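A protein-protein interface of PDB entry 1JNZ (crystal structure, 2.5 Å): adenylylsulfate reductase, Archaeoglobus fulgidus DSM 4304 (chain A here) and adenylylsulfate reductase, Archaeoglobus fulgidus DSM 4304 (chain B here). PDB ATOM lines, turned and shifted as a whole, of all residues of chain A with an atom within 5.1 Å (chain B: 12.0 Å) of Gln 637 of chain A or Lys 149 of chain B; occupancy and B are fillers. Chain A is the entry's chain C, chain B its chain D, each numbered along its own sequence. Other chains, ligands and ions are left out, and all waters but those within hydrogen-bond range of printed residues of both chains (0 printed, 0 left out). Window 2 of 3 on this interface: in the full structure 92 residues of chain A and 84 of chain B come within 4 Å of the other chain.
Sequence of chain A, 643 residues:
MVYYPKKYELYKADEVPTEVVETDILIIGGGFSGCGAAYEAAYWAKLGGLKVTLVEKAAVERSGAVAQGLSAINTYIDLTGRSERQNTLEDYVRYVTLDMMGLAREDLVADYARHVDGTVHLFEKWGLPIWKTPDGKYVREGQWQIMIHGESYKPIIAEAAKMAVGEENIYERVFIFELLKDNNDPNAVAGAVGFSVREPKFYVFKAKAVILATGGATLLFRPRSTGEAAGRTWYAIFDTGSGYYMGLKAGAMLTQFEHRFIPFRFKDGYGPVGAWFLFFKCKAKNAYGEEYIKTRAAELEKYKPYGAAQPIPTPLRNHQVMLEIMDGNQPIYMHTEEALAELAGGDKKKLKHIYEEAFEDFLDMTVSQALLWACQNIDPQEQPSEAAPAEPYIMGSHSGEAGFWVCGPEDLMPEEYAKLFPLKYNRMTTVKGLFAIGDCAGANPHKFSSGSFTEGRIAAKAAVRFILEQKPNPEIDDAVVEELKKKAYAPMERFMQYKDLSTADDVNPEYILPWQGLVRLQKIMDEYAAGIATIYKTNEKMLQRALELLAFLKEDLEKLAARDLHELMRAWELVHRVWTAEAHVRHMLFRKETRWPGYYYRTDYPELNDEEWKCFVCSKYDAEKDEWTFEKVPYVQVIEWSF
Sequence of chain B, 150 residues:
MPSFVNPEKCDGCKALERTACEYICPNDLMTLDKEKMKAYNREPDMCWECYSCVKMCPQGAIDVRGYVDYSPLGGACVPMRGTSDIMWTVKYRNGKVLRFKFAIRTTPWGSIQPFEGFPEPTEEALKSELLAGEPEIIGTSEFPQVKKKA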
ATOM      1  N   GLU A 106      -1.424  27.075  36.766  1.00  0.00           N
ATOM      2  CA  GLU A 106      -0.573  26.048  36.189  1.00  0.00           C
ATOM      3  C   GLU A 106       0.867  26.045  36.695  1.00  0.00           C
ATOM      4  O   GLU A 106       1.539  25.008  36.665  1.00  0.00           O
ATOM      5  CB  GLU A 106      -0.608  26.150  34.662  1.00  0.00           C
ATOM      6  CG  GLU A 106      -2.022  26.125  34.104  1.00  0.00           C
ATOM      7  CD  GLU A 106      -2.068  25.887  32.609  1.00  0.00           C
ATOM      8  OE1 GLU A 106      -1.082  26.226  31.917  1.00  0.00           O
ATOM      9  OE2 GLU A 106      -3.100  25.375  32.122  1.00  0.00           O
ATOM     10  N   TYR A 635      -6.342  34.646  33.801  1.00  0.00           N
ATOM     11  CA  TYR A 635      -5.628  33.388  33.725  1.00  0.00           C
ATOM     12  C   TYR A 635      -4.729  33.474  32.492  1.00  0.00           C
ATOM     13  O   TYR A 635      -5.069  34.146  31.518  1.00  0.00           O
ATOM     14  CB  TYR A 635      -6.632  32.237  33.558  1.00  0.00           C
ATOM     15  CG  TYR A 635      -6.086  31.016  32.845  1.00  0.00           C
ATOM     16  CD1 TYR A 635      -5.571  29.932  33.557  1.00  0.00           C
ATOM     17  CD2 TYR A 635      -6.075  30.956  31.449  1.00  0.00           C
ATOM     18  CE1 TYR A 635      -5.058  28.812  32.895  1.00  0.00           C
ATOM     19  CE2 TYR A 635      -5.563  29.851  30.777  1.00  0.00           C
ATOM     20  CZ  TYR A 635      -5.058  28.782  31.502  1.00  0.00           C
ATOM     21  OH  TYR A 635      -4.557  27.688  30.829  1.00  0.00           O
ATOM     22  N   VAL A 636      -3.577  32.815  32.548  1.00  0.00           N
ATOM     23  CA  VAL A 636      -2.668  32.753  31.411  1.00  0.00           C
ATOM     24  C   VAL A 636      -2.150  31.327  31.388  1.00  0.00           C
ATOM     25  O   VAL A 636      -1.806  30.775  32.435  1.00  0.00           O
ATOM     26  CB  VAL A 636      -1.458  33.724  31.538  1.00  0.00           C
ATOM     27  CG1 VAL A 636      -1.935  35.162  31.490  1.00  0.00           C
ATOM     28  CG2 VAL A 636      -0.693  33.459  32.818  1.00  0.00           C
ATOM     29  N   GLN A 637      -2.118  30.710  30.211  1.00  0.00           N
ATOM     30  CA  GLN A 637      -1.616  29.348  30.127  1.00  0.00           C
ATOM     31  C   GLN A 637      -0.101  29.414  30.295  1.00  0.00           C
ATOM     32  O   GLN A 637       0.589  30.128  29.567  1.00  0.00           O
ATOM     33  CB  GLN A 637      -1.973  28.703  28.787  1.00  0.00           C
ATOM     34  CG  GLN A 637      -1.761  27.194  28.792  1.00  0.00           C
ATOM     35  CD  GLN A 637      -2.175  26.528  27.493  1.00  0.00           C
ATOM     36  OE1 GLN A 637      -3.221  26.844  26.928  1.00  0.00           O
ATOM     37  NE2 GLN A 637      -1.364  25.583  27.024  1.00  0.00           N
ATOM     38  N   VAL A 638       0.404  28.671  31.272  1.00  0.00           N
ATOM     39  CA  VAL A 638       1.828  28.648  31.572  1.00  0.00           C
ATOM     40  C   VAL A 638       2.525  27.449  30.945  1.00  0.00           C
ATOM     41  O   VAL A 638       3.648  27.558  30.447  1.00  0.00           O
ATOM     42  CB  VAL A 638       2.054  28.608  33.100  1.00  0.00           C
ATOM     43  CG1 VAL A 638       3.540  28.519  33.405  1.00  0.00           C
ATOM     44  CG2 VAL A 638       1.436  29.843  33.747  1.00  0.00           C
ATOM     45  N   ILE A 639       1.849  26.308  30.969  1.00  0.00           N
ATOM     46  CA  ILE A 639       2.404  25.083  30.427  1.00  0.00           C
ATOM     47  C   ILE A 639       1.914  24.792  29.016  1.00  0.00           C
ATOM     48  O   ILE A 639       0.770  25.091  28.662  1.00  0.00           O
ATOM     49  CB  ILE A 639       2.064  23.889  31.351  1.00  0.00           C
ATOM     50  CG1 ILE A 639       2.680  24.123  32.740  1.00  0.00           C
ATOM     51  CG2 ILE A 639       2.549  22.587  30.744  1.00  0.00           C
ATOM     52  CD1 ILE A 639       4.178  24.350  32.731  1.00  0.00           C
ATOM     53  N   GLU A 640       2.797  24.207  28.213  1.00  0.00           N
ATOM     54  CA  GLU A 640       2.476  23.863  26.840  1.00  0.00           C
ATOM     55  C   GLU A 640       1.548  22.658  26.741  1.00  0.00           C
ATOM     56  O   GLU A 640       1.881  21.560  27.186  1.00  0.00           O
ATOM     57  CB  GLU A 640       3.756  23.579  26.048  1.00  0.00           C
ATOM     58  CG  GLU A 640       3.497  23.089  24.626  1.00  0.00           C
ATOM     59  CD  GLU A 640       4.773  22.846  23.843  1.00  0.00           C
ATOM     60  OE1 GLU A 640       5.541  23.812  23.634  1.00  0.00           O
ATOM     61  OE2 GLU A 640       5.013  21.686  23.434  1.00  0.00           O
ATOM     62  N   TRP A 641       0.376  22.883  26.157  1.00  0.00           N
ATOM     63  CA  TRP A 641      -0.617  21.834  25.941  1.00  0.00           C
ATOM     64  C   TRP A 641      -1.762  22.401  25.117  1.00  0.00           C
ATOM     65  O   TRP A 641      -1.995  23.612  25.104  1.00  0.00           O
ATOM     66  CB  TRP A 641      -1.159  21.278  27.267  1.00  0.00           C
ATOM     67  CG  TRP A 641      -1.902  22.265  28.125  1.00  0.00           C
ATOM     68  CD1 TRP A 641      -1.409  22.958  29.193  1.00  0.00           C
ATOM     69  CD2 TRP A 641      -3.278  22.653  27.999  1.00  0.00           C
ATOM     70  NE1 TRP A 641      -2.392  23.751  29.744  1.00  0.00           N
ATOM     71  CE2 TRP A 641      -3.548  23.585  29.027  1.00  0.00           C
ATOM     72  CE3 TRP A 641      -4.310  22.307  27.112  1.00  0.00           C
ATOM     73  CZ2 TRP A 641      -4.807  24.172  29.199  1.00  0.00           C
ATOM     74  CZ3 TRP A 641      -5.568  22.895  27.284  1.00  0.00           C
ATOM     75  CH2 TRP A 641      -5.801  23.817  28.320  1.00  0.00           C
ATOM     76  N   SER A 642      -2.470  21.520  24.421  1.00  0.00           N
ATOM     77  CA  SER A 642      -3.593  21.925  23.591  1.00  0.00           C
ATOM     78  C   SER A 642      -4.734  20.934  23.775  1.00  0.00           C
ATOM     79  O   SER A 642      -4.512  19.761  24.065  1.00  0.00           O
ATOM     80  CB  SER A 642      -3.181  21.955  22.118  1.00  0.00           C
ATOM     81  OG  SER A 642      -2.890  20.644  21.663  1.00  0.00           O
ATOM     82  N   GLN B 145      11.493  17.816  33.837  1.00  0.00           N
ATOM     83  CA  GLN B 145      11.296  19.073  33.127  1.00  0.00           C
ATOM     84  C   GLN B 145       9.847  19.118  32.656  1.00  0.00           C
ATOM     85  O   GLN B 145       9.231  18.078  32.424  1.00  0.00           O
ATOM     86  CB  GLN B 145      12.231  19.155  31.913  1.00  0.00           C
ATOM     87  CG  GLN B 145      13.715  19.191  32.246  1.00  0.00           C
ATOM     88  CD  GLN B 145      14.119  20.461  32.970  1.00  0.00           C
ATOM     89  OE1 GLN B 145      13.991  21.562  32.433  1.00  0.00           O
ATOM     90  NE2 GLN B 145      14.605  20.316  34.197  1.00  0.00           N
ATOM     91  N   VAL B 146       9.299  20.318  32.530  1.00  0.00           N
ATOM     92  CA  VAL B 146       7.931  20.469  32.061  1.00  0.00           C
ATOM     93  C   VAL B 146       7.966  21.589  31.023  1.00  0.00           C
ATOM     94  O   VAL B 146       8.516  22.662  31.274  1.00  0.00           O
ATOM     95  CB  VAL B 146       6.971  20.797  33.231  1.00  0.00           C
ATOM     96  CG1 VAL B 146       7.397  22.085  33.920  1.00  0.00           C
ATOM     97  CG2 VAL B 146       5.537  20.875  32.722  1.00  0.00           C
ATOM     98  N   LYS B 147       7.394  21.331  29.849  1.00  0.00           N
ATOM     99  CA  LYS B 147       7.431  22.316  28.776  1.00  0.00           C
ATOM    100  C   LYS B 147       6.587  23.528  29.054  1.00  0.00           C
ATOM    101  O   LYS B 147       5.382  23.430  29.283  1.00  0.00           O
ATOM    102  CB  LYS B 147       6.960  21.712  27.458  1.00  0.00           C
ATOM    103  CG  LYS B 147       7.764  20.488  27.032  1.00  0.00           C
ATOM    104  CD  LYS B 147       7.204  19.900  25.738  1.00  0.00           C
ATOM    105  CE  LYS B 147       7.944  18.634  25.320  1.00  0.00           C
ATOM    106  NZ  LYS B 147       7.825  17.565  26.352  1.00  0.00           N
ATOM    107  N   LYS B 148       7.231  24.683  29.021  1.00  0.00           N
ATOM    108  CA  LYS B 148       6.527  25.919  29.239  1.00  0.00           C
ATOM    109  C   LYS B 148       5.934  26.355  27.935  1.00  0.00           C
ATOM    110  O   LYS B 148       6.496  26.112  26.863  1.00  0.00           O
ATOM    111  CB  LYS B 148       7.469  26.972  29.767  1.00  0.00           C
ATOM    112  CG  LYS B 148       7.602  26.854  31.240  1.00  0.00           C
ATOM    113  CD  LYS B 148       8.583  27.840  31.765  1.00  0.00           C
ATOM    114  CE  LYS B 148       7.873  29.067  32.234  1.00  0.00           C
ATOM    115  NZ  LYS B 148       8.880  29.944  32.857  1.00  0.00           N
ATOM    116  N   LYS B 149       4.787  27.002  28.022  1.00  0.00           N
ATOM    117  CA  LYS B 149       4.144  27.432  26.818  1.00  0.00           C
ATOM    118  C   LYS B 149       4.870  28.597  26.161  1.00  0.00           C
ATOM    119  O   LYS B 149       5.162  29.607  26.803  1.00  0.00           O
ATOM    120  CB  LYS B 149       2.693  27.795  27.085  1.00  0.00           C
ATOM    121  CG  LYS B 149       1.997  27.785  25.759  1.00  0.00           C
ATOM    122  CD  LYS B 149       0.804  28.651  25.762  1.00  0.00           C
ATOM    123  CE  LYS B 149       0.244  28.673  24.379  1.00  0.00           C
ATOM    124  NZ  LYS B 149      -0.462  29.949  24.203  1.00  0.00           N
ATOM    125  N   ALA B 150       5.175  28.450  24.874  1.00  0.00           N
ATOM    126  CA  ALA B 150       5.873  29.486  24.120  1.00  0.00           C
ATOM    127  C   ALA B 150       5.066  30.778  24.075  1.00  0.00           C
ATOM    128  O   ALA B 150       4.341  30.982  23.075  1.00  0.00           O
ATOM    129  CB  ALA B 150       6.161  29.000  22.710  1.00  0.00           C
ATOM    130  OXT ALA B 150       5.149  31.563  25.045  1.00  0.00           O
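The backbone carbonyl oxygen of Val 638 of chain A sits at hydrogen-bond distance from the backbone NH of Lys 149 of chain B, 2.7 Å away. The backbone NH (N) of Glu 640 of chain A lies close to the backbone NH (N) of Lys 149 of chain B, at 3.4 Å. The backbone carbonyl oxygen of Lys 147 of chain B is in hydrogen-bond range of the backbone NH of Glu 640 of chain A, at 2.9 Å.
N of Val 638 of chain A lies within hydrogen-bond range of OE1 of Glu 106 of chain A, 2.9 Å away. NE2 of Gln 637 of chain A lies within hydrogen-bond range of O of Ile 639 of chain A (2.7 Å). O of Trp 641 of chain A is in hydrogen-bond range of NE2 of Gln 637 of chain A (2.8 Å). OE1 of Glu 106 of chain A sits at hydrogen-bond distance from N of Ile 639 of chain A, 3.1 Å away.
Among the printed residues, pairs that only touch across the chains: Ile 639 of chain A with Lys 147 of chain B, Val 638 of chain A with Lys 148 of chain B, Ile 639 of chain A with Lys 149 of chain B, Ile 639 of chain A with Val 146 of chain B, Glu 640 of chain A with Lys 148 of chain B and Gln 637 of chain A with Lys 149 of chain B.
No residue of chain B comes within 4 Å of Glu 106 of chain A. No residue of chain B comes within 4 Å of Tyr 635 of chain A. No residue of chain B comes within 4 Å of Val 636 of chain A. Glu 640 of chain A touches three residues of chain B. Of the printed residues of chain A, Val 146 of chain B touches Ile 639. Printed residues of chain A within 4 Å of Lys 147 of chain B: Ile 639 and Glu 640. Printed residues of chain A within 4 Å of Lys 148 of chain B: Val 638 and Glu 640. The nearest residue of chain B that does not touch Gln 637 of chain A is Ala 150 of chain B (6.6 Å). The nearest printed residue of chain A that does not touch Val 146 of chain B is Glu 640 of chain A (6.2 Å).
Of the 9 printed residues of chain A, 4 touch a printed residue of chain B. Hydrophobic or aromatic side chains of chain A within 4 Å of the printed part of chain B: Ile 639. Printed residues of chain B that touch a printed residue of chain A: Val 146, Lys 147, Lys 148 and Lys 149. Hydrophobic or aromatic side chains of chain B that line the printed part of chain A: Val 146. Among the printed residues, 9 pairs touch across the chains. Among the printed residues, no Asp or Glu carboxylate lies within 4 Å of a Lys or Arg side-chain nitrogen of the other chain.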
